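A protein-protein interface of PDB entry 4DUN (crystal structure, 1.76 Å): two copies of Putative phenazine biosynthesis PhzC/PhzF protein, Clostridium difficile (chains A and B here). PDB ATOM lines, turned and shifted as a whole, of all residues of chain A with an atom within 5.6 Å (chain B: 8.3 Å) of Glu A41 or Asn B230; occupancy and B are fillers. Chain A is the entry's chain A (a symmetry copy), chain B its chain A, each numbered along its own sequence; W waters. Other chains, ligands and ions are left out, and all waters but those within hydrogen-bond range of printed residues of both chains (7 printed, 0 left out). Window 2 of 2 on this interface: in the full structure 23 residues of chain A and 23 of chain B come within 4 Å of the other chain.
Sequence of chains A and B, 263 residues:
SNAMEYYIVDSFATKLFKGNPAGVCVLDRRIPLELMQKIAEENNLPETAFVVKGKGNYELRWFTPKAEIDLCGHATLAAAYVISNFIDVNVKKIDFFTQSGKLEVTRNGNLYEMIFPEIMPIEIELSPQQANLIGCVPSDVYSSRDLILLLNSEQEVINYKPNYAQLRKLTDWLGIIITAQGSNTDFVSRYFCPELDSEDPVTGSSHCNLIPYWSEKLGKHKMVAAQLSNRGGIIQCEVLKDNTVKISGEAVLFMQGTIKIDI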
ATOM      1  N   MET A  36      -3.712  -7.809  18.226  1.00  0.00           N
ATOM      2  CA  MET A  36      -3.390  -8.574  17.014  1.00  0.00           C
ATOM      3  C   MET A  36      -4.025  -7.884  15.802  1.00  0.00           C
ATOM      4  O   MET A  36      -3.363  -7.733  14.773  1.00  0.00           O
ATOM      5  CB  MET A  36      -3.854 -10.042  17.114  1.00  0.00           C
ATOM      6  CG  MET A  36      -3.094 -10.846  18.129  1.00  0.00           C
ATOM      7  SD  MET A  36      -3.748 -12.532  18.123  1.00  0.00           S
ATOM      8  CE  MET A  36      -2.996 -13.160  19.647  1.00  0.00           C
ATOM      9  N   GLN A  37      -5.299  -7.418  15.938  1.00  0.00           N
ATOM     10  CA  GLN A  37      -5.982  -6.723  14.852  1.00  0.00           C
ATOM     11  C   GLN A  37      -5.243  -5.434  14.472  1.00  0.00           C
ATOM     12  O   GLN A  37      -5.073  -5.168  13.274  1.00  0.00           O
ATOM     13  CB  GLN A  37      -7.453  -6.396  15.218  1.00  0.00           C
ATOM     14  CG  GLN A  37      -8.227  -5.767  14.041  1.00  0.00           C
ATOM     15  CD  GLN A  37      -8.287  -6.698  12.854  1.00  0.00           C
ATOM     16  OE1 GLN A  37      -9.076  -7.635  12.836  1.00  0.00           O
ATOM     17  NE2 GLN A  37      -7.440  -6.473  11.845  1.00  0.00           N
ATOM     18  N   LYS A  38      -4.817  -4.626  15.477  1.00  0.00           N
ATOM     19  CA  LYS A  38      -4.091  -3.365  15.195  1.00  0.00           C
ATOM     20  C   LYS A  38      -2.808  -3.639  14.442  1.00  0.00           C
ATOM     21  O   LYS A  38      -2.480  -2.905  13.492  1.00  0.00           O
ATOM     22  CB  LYS A  38      -3.780  -2.573  16.484  1.00  0.00           C
ATOM     23  CG  LYS A  38      -5.006  -1.920  17.174  1.00  0.00           C
ATOM     24  CD  LYS A  38      -5.957  -1.163  16.229  1.00  0.00           C
ATOM     25  CE  LYS A  38      -5.545   0.258  15.940  1.00  0.00           C
ATOM     26  NZ  LYS A  38      -6.479   0.906  14.983  1.00  0.00           N
ATOM     27  N   ILE A  39      -2.096  -4.709  14.843  1.00  0.00           N
ATOM     28  CA  ILE A  39      -0.842  -5.126  14.195  1.00  0.00           C
ATOM     29  C   ILE A  39      -1.112  -5.525  12.743  1.00  0.00           C
ATOM     30  O   ILE A  39      -0.368  -5.092  11.858  1.00  0.00           O
ATOM     31  CB  ILE A  39      -0.099  -6.250  14.978  1.00  0.00           C
ATOM     32  CG1 ILE A  39       0.478  -5.669  16.297  1.00  0.00           C
ATOM     33  CG2 ILE A  39       1.028  -6.925  14.110  1.00  0.00           C
ATOM     34  CD1 ILE A  39       0.777  -6.756  17.399  1.00  0.00           C
ATOM     35  N   ALA A  40      -2.183  -6.303  12.495  1.00  0.00           N
ATOM     36  CA  ALA A  40      -2.539  -6.739  11.125  1.00  0.00           C
ATOM     37  C   ALA A  40      -2.910  -5.527  10.247  1.00  0.00           C
ATOM     38  O   ALA A  40      -2.528  -5.492   9.075  1.00  0.00           O
ATOM     39  CB  ALA A  40      -3.677  -7.749  11.168  1.00  0.00           C
ATOM     40  N   GLU A  41      -3.608  -4.539  10.823  1.00  0.00           N
ATOM     41  CA  GLU A  41      -3.996  -3.311  10.138  1.00  0.00           C
ATOM     42  C   GLU A  41      -2.749  -2.465   9.798  1.00  0.00           C
ATOM     43  O   GLU A  41      -2.686  -1.872   8.713  1.00  0.00           O
ATOM     44  CB  GLU A  41      -4.981  -2.526  11.016  1.00  0.00           C
ATOM     45  CG  GLU A  41      -5.661  -1.372  10.301  1.00  0.00           C
ATOM     46  CD  GLU A  41      -6.558  -0.510  11.168  1.00  0.00           C
ATOM     47  OE1 GLU A  41      -6.954  -0.951  12.273  1.00  0.00           O
ATOM     48  OE2 GLU A  41      -6.867   0.622  10.729  1.00  0.00           O
ATOM     49  N   GLU A  42      -1.772  -2.417  10.724  1.00  0.00           N
ATOM     50  CA  GLU A  42      -0.512  -1.678  10.571  1.00  0.00           C
ATOM     51  C   GLU A  42       0.351  -2.303   9.456  1.00  0.00           C
ATOM     52  O   GLU A  42       0.881  -1.578   8.604  1.00  0.00           O
ATOM     53  CB  GLU A  42       0.251  -1.625  11.912  1.00  0.00           C
ATOM     54  CG  GLU A  42       1.537  -0.805  11.856  1.00  0.00           C
ATOM     55  CD  GLU A  42       1.422   0.706  11.832  1.00  0.00           C
ATOM     56  OE1 GLU A  42       0.295   1.235  11.953  1.00  0.00           O
ATOM     57  OE2 GLU A  42       2.487   1.358  11.734  1.00  0.00           O
ATOM     58  N   ASN A  43       0.445  -3.639   9.432  1.00  0.00           N
ATOM     59  CA  ASN A  43       1.180  -4.342   8.387  1.00  0.00           C
ATOM     60  C   ASN A  43       0.553  -4.129   6.999  1.00  0.00           C
ATOM     61  O   ASN A  43       1.279  -3.991   6.003  1.00  0.00           O
ATOM     62  CB  ASN A  43       1.238  -5.828   8.703  1.00  0.00           C
ATOM     63  CG  ASN A  43       2.188  -6.131   9.824  1.00  0.00           C
ATOM     64  OD1 ASN A  43       3.185  -5.439  10.026  1.00  0.00           O
ATOM     65  ND2 ASN A  43       1.930  -7.222  10.542  1.00  0.00           N
ATOM     66  N   ASN A  44      -0.792  -4.098   6.944  1.00  0.00           N
ATOM     67  CA  ASN A  44      -1.582  -3.949   5.719  1.00  0.00           C
ATOM     68  C   ASN A  44      -1.299  -5.074   4.695  1.00  0.00           C
ATOM     69  O   ASN A  44      -1.540  -4.909   3.495  1.00  0.00           O
ATOM     70  CB  ASN A  44      -1.387  -2.569   5.064  1.00  0.00           C
ATOM     71  CG  ASN A  44      -2.561  -2.212   4.191  1.00  0.00           C
ATOM     72  OD1 ASN A  44      -3.723  -2.510   4.534  1.00  0.00           O
ATOM     73  ND2 ASN A  44      -2.284  -1.666   3.009  1.00  0.00           N
ATOM     74  N   THR A  64      -6.898 -10.427   8.783  1.00  0.00           N
ATOM     75  CA  THR A  64      -6.721  -9.563   7.618  1.00  0.00           C
ATOM     76  C   THR A  64      -6.523  -8.145   8.214  1.00  0.00           C
ATOM     77  O   THR A  64      -6.728  -7.986   9.425  1.00  0.00           O
ATOM     78  CB  THR A  64      -7.954  -9.618   6.681  1.00  0.00           C
ATOM     79  OG1 THR A  64      -9.047  -8.997   7.365  1.00  0.00           O
ATOM     80  CG2 THR A  64      -8.307 -11.044   6.210  1.00  0.00           C
ATOM     81  N   PRO A  65      -6.302  -7.082   7.419  1.00  0.00           N
ATOM     82  CA  PRO A  65      -6.233  -5.733   8.020  1.00  0.00           C
ATOM     83  C   PRO A  65      -7.569  -5.279   8.662  1.00  0.00           C
ATOM     84  O   PRO A  65      -7.594  -4.248   9.343  1.00  0.00           O
ATOM     85  CB  PRO A  65      -5.898  -4.848   6.815  1.00  0.00           C
ATOM     86  CG  PRO A  65      -5.141  -5.772   5.879  1.00  0.00           C
ATOM     87  CD  PRO A  65      -5.961  -7.042   5.978  1.00  0.00           C
ATOM     88  N   PHE B  17       0.076   3.065  15.879  1.00  0.00           N
ATOM     89  CA  PHE B  17      -1.142   2.815  15.062  1.00  0.00           C
ATOM     90  C   PHE B  17      -1.916   4.100  14.693  1.00  0.00           C
ATOM     91  O   PHE B  17      -3.029   4.028  14.148  1.00  0.00           O
ATOM     92  CB  PHE B  17      -2.095   1.820  15.742  1.00  0.00           C
ATOM     93  CG  PHE B  17      -1.397   0.576  16.241  1.00  0.00           C
ATOM     94  CD1 PHE B  17      -0.640  -0.211  15.378  1.00  0.00           C
ATOM     95  CD2 PHE B  17      -1.496   0.194  17.572  1.00  0.00           C
ATOM     96  CE1 PHE B  17       0.005  -1.364  15.834  1.00  0.00           C
ATOM     97  CE2 PHE B  17      -0.868  -0.974  18.031  1.00  0.00           C
ATOM     98  CZ  PHE B  17      -0.116  -1.742  17.163  1.00  0.00           C
ATOM     99  N   LYS B  18      -1.328   5.255  14.987  1.00  0.00           N
ATOM    100  CA  LYS B  18      -1.897   6.551  14.649  1.00  0.00           C
ATOM    101  C   LYS B  18      -1.046   7.160  13.540  1.00  0.00           C
ATOM    102  O   LYS B  18      -0.077   6.538  13.068  1.00  0.00           O
ATOM    103  CB  LYS B  18      -1.966   7.460  15.896  1.00  0.00           C
ATOM    104  CG  LYS B  18      -2.898   6.905  16.991  1.00  0.00           C
ATOM    105  CD  LYS B  18      -3.247   7.966  18.027  1.00  0.00           C
ATOM    106  CE  LYS B  18      -4.156   7.433  19.103  1.00  0.00           C
ATOM    107  NZ  LYS B  18      -5.560   7.313  18.627  1.00  0.00           N
ATOM    108  N   GLY B  19      -1.435   8.336  13.084  1.00  0.00           N
ATOM    109  CA  GLY B  19      -0.674   9.036  12.060  1.00  0.00           C
ATOM    110  C   GLY B  19      -0.675   8.367  10.701  1.00  0.00           C
ATOM    111  O   GLY B  19      -1.542   7.526  10.411  1.00  0.00           O
ATOM    112  N   PRO B  21       1.326   5.907   8.180  1.00  0.00           N
ATOM    113  CA  PRO B  21       2.424   4.921   8.192  1.00  0.00           C
ATOM    114  C   PRO B  21       3.266   4.888   6.908  1.00  0.00           C
ATOM    115  O   PRO B  21       2.744   4.993   5.792  1.00  0.00           O
ATOM    116  CB  PRO B  21       1.704   3.585   8.421  1.00  0.00           C
ATOM    117  CG  PRO B  21       0.361   3.781   7.774  1.00  0.00           C
ATOM    118  CD  PRO B  21       0.017   5.259   7.948  1.00  0.00           C
ATOM    119  N   ASN B  44       3.357  -3.043   0.733  1.00  0.00           N
ATOM    120  CA  ASN B  44       1.957  -2.637   0.589  1.00  0.00           C
ATOM    121  C   ASN B  44       1.575  -1.488   1.551  1.00  0.00           C
ATOM    122  O   ASN B  44       0.395  -1.292   1.864  1.00  0.00           O
ATOM    123  CB  ASN B  44       0.987  -3.821   0.760  1.00  0.00           C
ATOM    124  CG  ASN B  44      -0.328  -3.548   0.077  1.00  0.00           C
ATOM    125  OD1 ASN B  44      -0.363  -2.947  -1.015  1.00  0.00           O
ATOM    126  ND2 ASN B  44      -1.429  -3.885   0.743  1.00  0.00           N
ATOM    127  N   LEU B  45       2.575  -0.719   2.003  1.00  0.00           N
ATOM    128  CA  LEU B  45       2.314   0.449   2.824  1.00  0.00           C
ATOM    129  C   LEU B  45       2.035   1.644   1.879  1.00  0.00           C
ATOM    130  O   LEU B  45       2.448   1.598   0.720  1.00  0.00           O
ATOM    131  CB  LEU B  45       3.475   0.713   3.806  1.00  0.00           C
ATOM    132  CG  LEU B  45       3.617  -0.318   4.931  1.00  0.00           C
ATOM    133  CD1 LEU B  45       4.902  -0.092   5.726  1.00  0.00           C
ATOM    134  CD2 LEU B  45       2.384  -0.306   5.857  1.00  0.00           C
ATOM    135  N   PRO B  46       1.302   2.693   2.329  1.00  0.00           N
ATOM    136  CA  PRO B  46       0.958   3.820   1.428  1.00  0.00           C
ATOM    137  C   PRO B  46       2.162   4.340   0.628  1.00  0.00           C
ATOM    138  O   PRO B  46       2.057   4.592  -0.578  1.00  0.00           O
ATOM    139  CB  PRO B  46       0.421   4.877   2.386  1.00  0.00           C
ATOM    140  CG  PRO B  46      -0.221   4.060   3.487  1.00  0.00           C
ATOM    141  CD  PRO B  46       0.702   2.877   3.677  1.00  0.00           C
ATOM    142  N   ARG B 190      -9.964  16.954   7.491  1.00  0.00           N
ATOM    143  CA  ARG B 190      -9.907  15.630   6.890  1.00  0.00           C
ATOM    144  C   ARG B 190      -9.601  15.866   5.416  1.00  0.00           C
ATOM    145  O   ARG B 190     -10.071  16.853   4.837  1.00  0.00           O
ATOM    146  CB  ARG B 190     -11.174  14.806   7.109  1.00  0.00           C
ATOM    147  CG  ARG B 190     -11.332  14.338   8.563  1.00  0.00           C
ATOM    148  CD  ARG B 190     -12.696  13.758   8.793  1.00  0.00           C
ATOM    149  NE  ARG B 190     -12.844  12.468   8.128  1.00  0.00           N
ATOM    150  CZ  ARG B 190     -14.004  11.867   7.900  1.00  0.00           C
ATOM    151  NH1 ARG B 190     -15.150  12.443   8.279  1.00  0.00           N
ATOM    152  NH2 ARG B 190     -14.036  10.690   7.292  1.00  0.00           N
ATOM    153  N   GLU B 199      -9.001   8.113   2.232  1.00  0.00           N
ATOM    154  CA  GLU B 199      -8.846   9.290   3.075  1.00  0.00           C
ATOM    155  C   GLU B 199      -7.403   9.318   3.565  1.00  0.00           C
ATOM    156  O   GLU B 199      -6.909   8.329   4.097  1.00  0.00           O
ATOM    157  CB  GLU B 199      -9.841   9.268   4.238  1.00  0.00           C
ATOM    158  CG  GLU B 199      -9.559  10.368   5.241  1.00  0.00           C
ATOM    159  CD  GLU B 199     -10.526  10.444   6.402  1.00  0.00           C
ATOM    160  OE1 GLU B 199     -11.407   9.564   6.524  1.00  0.00           O
ATOM    161  OE2 GLU B 199     -10.381  11.386   7.208  1.00  0.00           O
ATOM    162  N   ASP B 200      -6.714  10.436   3.359  1.00  0.00           N
ATOM    163  CA  ASP B 200      -5.315  10.534   3.775  1.00  0.00           C
ATOM    164  C   ASP B 200      -5.234  10.605   5.317  1.00  0.00           C
ATOM    165  O   ASP B 200      -5.912  11.437   5.912  1.00  0.00           O
ATOM    166  CB  ASP B 200      -4.715  11.796   3.152  1.00  0.00           C
ATOM    167  CG  ASP B 200      -3.212  11.817   3.019  1.00  0.00           C
ATOM    168  OD1 ASP B 200      -2.572  10.725   3.141  1.00  0.00           O
ATOM    169  OD2 ASP B 200      -2.674  12.893   2.734  1.00  0.00           O
ATOM    170  N   PRO B 201      -4.459   9.716   5.981  1.00  0.00           N
ATOM    171  CA  PRO B 201      -4.383   9.757   7.456  1.00  0.00           C
ATOM    172  C   PRO B 201      -3.924  11.122   8.000  1.00  0.00           C
ATOM    173  O   PRO B 201      -4.561  11.655   8.906  1.00  0.00           O
ATOM    174  CB  PRO B 201      -3.380   8.644   7.783  1.00  0.00           C
ATOM    175  CG  PRO B 201      -3.549   7.669   6.626  1.00  0.00           C
ATOM    176  CD  PRO B 201      -3.660   8.599   5.440  1.00  0.00           C
ATOM    177  N   VAL B 202      -2.823  11.672   7.471  1.00  0.00           N
ATOM    178  CA  VAL B 202      -2.278  12.980   7.880  1.00  0.00           C
ATOM    179  C   VAL B 202      -1.665  13.629   6.650  1.00  0.00           C
ATOM    180  O   VAL B 202      -0.884  12.983   5.944  1.00  0.00           O
ATOM    181  CB  VAL B 202      -1.245  12.971   9.054  1.00  0.00           C
ATOM    182  CG1 VAL B 202      -1.126  14.368   9.667  1.00  0.00           C
ATOM    183  CG2 VAL B 202      -1.606  11.962  10.139  1.00  0.00           C
ATOM    184  N   GLN B 227      -5.885  16.137  12.376  1.00  0.00           N
ATOM    185  CA  GLN B 227      -6.430  15.561  11.154  1.00  0.00           C
ATOM    186  C   GLN B 227      -7.269  14.401  11.645  1.00  0.00           C
ATOM    187  O   GLN B 227      -6.724  13.472  12.246  1.00  0.00           O
ATOM    188  CB  GLN B 227      -5.345  15.158  10.136  1.00  0.00           C
ATOM    189  CG  GLN B 227      -6.003  14.796   8.798  1.00  0.00           C
ATOM    190  CD  GLN B 227      -5.138  15.065   7.601  1.00  0.00           C
ATOM    191  OE1 GLN B 227      -4.351  16.025   7.566  1.00  0.00           O
ATOM    192  NE2 GLN B 227      -5.281  14.227   6.578  1.00  0.00           N
ATOM    193  N   LEU B 228      -8.599  14.511  11.495  1.00  0.00           N
ATOM    194  CA  LEU B 228      -9.546  13.577  12.088  1.00  0.00           C
ATOM    195  C   LEU B 228      -9.856  12.369  11.198  1.00  0.00           C
ATOM    196  O   LEU B 228     -11.016  12.001  10.984  1.00  0.00           O
ATOM    197  CB  LEU B 228     -10.828  14.342  12.504  1.00  0.00           C
ATOM    198  CG  LEU B 228     -10.623  15.452  13.553  1.00  0.00           C
ATOM    199  CD1 LEU B 228     -11.955  16.120  13.885  1.00  0.00           C
ATOM    200  CD2 LEU B 228      -9.933  14.918  14.856  1.00  0.00           C
ATOM    201  N   SER B 229      -8.793  11.712  10.725  1.00  0.00           N
ATOM    202  CA  SER B 229      -8.883  10.450   9.997  1.00  0.00           C
ATOM    203  C   SER B 229      -9.083   9.343  11.040  1.00  0.00           C
ATOM    204  O   SER B 229      -8.925   9.617  12.237  1.00  0.00           O
ATOM    205  CB  SER B 229      -7.594  10.218   9.203  1.00  0.00           C
ATOM    206  OG  SER B 229      -6.488  10.261  10.096  1.00  0.00           O
ATOM    207  N   ASN B 230      -9.355   8.110  10.600  1.00  0.00           N
ATOM    208  CA  ASN B 230      -9.506   6.930  11.464  1.00  0.00           C
ATOM    209  C   ASN B 230      -8.277   6.802  12.384  1.00  0.00           C
ATOM    210  O   ASN B 230      -8.423   6.711  13.600  1.00  0.00           O
ATOM    211  CB  ASN B 230      -9.665   5.669  10.584  1.00  0.00           C
ATOM    212  CG  ASN B 230      -9.899   4.380  11.338  1.00  0.00           C
ATOM    213  OD1 ASN B 230     -10.495   4.350  12.426  1.00  0.00           O
ATOM    214  ND2 ASN B 230      -9.442   3.278  10.760  1.00  0.00           N
ATOM    215  N   ARG B 231      -7.070   6.883  11.796  1.00  0.00           N
ATOM    216  CA  ARG B 231      -5.813   6.794  12.540  1.00  0.00           C
ATOM    217  C   ARG B 231      -5.559   8.075  13.347  1.00  0.00           C
ATOM    218  O   ARG B 231      -5.184   7.989  14.521  1.00  0.00           O
ATOM    219  CB  ARG B 231      -4.648   6.491  11.589  1.00  0.00           C
ATOM    220  CG  ARG B 231      -4.753   5.082  10.953  1.00  0.00           C
ATOM    221  CD  ARG B 231      -3.609   4.818   9.984  1.00  0.00           C
ATOM    222  NE  ARG B 231      -2.311   4.869  10.657  1.00  0.00           N
ATOM    223  CZ  ARG B 231      -1.612   3.815  11.067  1.00  0.00           C
ATOM    224  NH1 ARG B 231      -2.059   2.582  10.846  1.00  0.00           N
ATOM    225  NH2 ARG B 231      -0.454   3.983  11.685  1.00  0.00           N
ATOM    226  N   GLY B 232      -5.805   9.222  12.720  1.00  0.00           N
ATOM    227  CA  GLY B 232      -5.688  10.542  13.332  1.00  0.00           C
ATOM    228  C   GLY B 232      -4.283  11.085  13.374  1.00  0.00           C
ATOM    229  O   GLY B 232      -3.313  10.342  13.540  1.00  0.00           O
ATOM    230  N   GLY B 233      -4.175  12.392  13.218  1.00  0.00           N
ATOM    231  CA  GLY B 233      -2.878  13.047  13.270  1.00  0.00           C
ATOM    232  C   GLY B 233      -2.911  14.349  14.028  1.00  0.00           C
ATOM    233  O   GLY B 233      -3.960  14.979  14.136  1.00  0.00           O
ATOM    234  N   PHE B 254       7.261   1.362  14.637  1.00  0.00           N
ATOM    235  CA  PHE B 254       6.436   0.163  14.785  1.00  0.00           C
ATOM    236  C   PHE B 254       7.293  -1.102  14.688  1.00  0.00           C
ATOM    237  O   PHE B 254       7.123  -2.026  15.477  1.00  0.00           O
ATOM    238  CB  PHE B 254       5.309   0.119  13.714  1.00  0.00           C
ATOM    239  CG  PHE B 254       4.630  -1.235  13.597  1.00  0.00           C
ATOM    240  CD1 PHE B 254       3.895  -1.759  14.661  1.00  0.00           C
ATOM    241  CD2 PHE B 254       4.707  -1.970  12.416  1.00  0.00           C
ATOM    242  CE1 PHE B 254       3.244  -2.997  14.542  1.00  0.00           C
ATOM    243  CE2 PHE B 254       4.052  -3.209  12.295  1.00  0.00           C
ATOM    244  CZ  PHE B 254       3.333  -3.715  13.361  1.00  0.00           C
HETATM  245  O   HOH W   1      -3.442  -6.348   1.927  1.00  0.00           O
HETATM  246  O   HOH W   2      -1.164   1.023   1.267  1.00  0.00           O
HETATM  247  O   HOH W   3      -7.896   3.472  13.735  1.00  0.00           O
HETATM  248  O   HOH W   4      -7.030   3.428   8.774  1.00  0.00           O
HETATM  249  O   HOH W   5      -4.727   1.786   9.077  1.00  0.00           O
HETATM  250  O   HOH W   6      -5.277   3.839  15.644  1.00  0.00           O
HETATM  251  O   HOH W   7      -4.794   1.984  13.183  1.00  0.00           O
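The guanidinium group of Arg B231 lies within salt-bridge range of the side-chain carboxylate of Glu A42, 2.9 Å away.
O of Asn B44 sits at hydrogen-bond distance from ND2 of Asn A44 (2.9 Å).
The side-chain amino group (NZ) of Lys A38 lies within salt-bridge range of the side-chain carboxylate (OE1) of Glu A41.
The backbone carbonyl oxygen (O) of Ile A39 lies within hydrogen-bond range of the side-chain amide nitrogen (ND2) of Asn A43.
The backbone carbonyl oxygen of Gly B19 is in hydrogen-bond range of the guanidinium group of Arg B231, at 2.8 Å.
The backbone carbonyl oxygen of Lys B18 is in hydrogen-bond range of the guanidinium group of Arg B231, at 2.9 Å.
Lys A38 touches Phe B17 (CB to CE2, 3.7 Å).
OE2 of Glu A41 touches ND2 of Asn B230, 3.7 Å away.
Glu A42 touches Phe B17.
CD2 of Leu B45 touches O of Glu A42, 3.4 Å away.
Glu A42 touches Phe B254 (CG to CD2, 3.4 Å).
Leu B45 touches Asn A43.
CE2 of Phe B254 touches OD1 of Asn A43, at 3.3 Å.
Printed residues of chain B within 4 Å of Glu A41: Asn B230 (3.7 Å).
Of the printed residues of chain A, Asn B230 touches Glu A41 (3.7 Å).
Printed residues of chain A within 4 Å of Phe B254: Glu A42 and Asn A43.
Printed residues of chain B within 4 Å of Lys A38: Phe B17 (3.7 Å).
Printed residues of chain B within 4 Å of Glu A42: Phe B17, Leu B45, Arg B231 and Phe B254.
The nearest printed residue of chain B that does not touch Glu A41 is Arg B231 (4.9 Å).
The nearest printed residue of chain A that does not touch Asn B230 is Lys A38 (5.7 Å).
Of the 11 printed residues of chain A, 5 touch a printed residue of chain B.
Printed residues of chain A that touch a printed residue of chain B: Lys A38, Glu A41, Glu A42, Asn A43 and Asn A44.
Of the 20 printed residues of chain B, 6 touch a printed residue of chain A.
Along chain B the printed residues that touch a printed residue of chain A span positions 17 to 254.
Among the printed residues, 9 pairs touch across the chains.
Asn A44 touches its own counterpart, Asn B44.
Water W7 lies within hydrogen-bond range of NZ of Lys A38, O of Phe B17 and OE2 of Glu A41.
Water W6 bridges O of Phe B17 and NZ of Lys A38.
Water W2 bridges O of Asn B44 (2.9 Å) and ND2 of Asn A44 (3.4 Å).
Water W1 bridges the backbone carbonyl oxygen of Asn A44 and the side-chain amide nitrogen of Asn B44.
Water W5 lies within hydrogen-bond range of the side-chain carboxylate (OE2) of Glu A41 and the guanidinium group (NH1) of Arg B231.
Water W3 bridges OD1 of Asn B230 (3.0 Å) and NZ of Lys A38 (3.2 Å).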
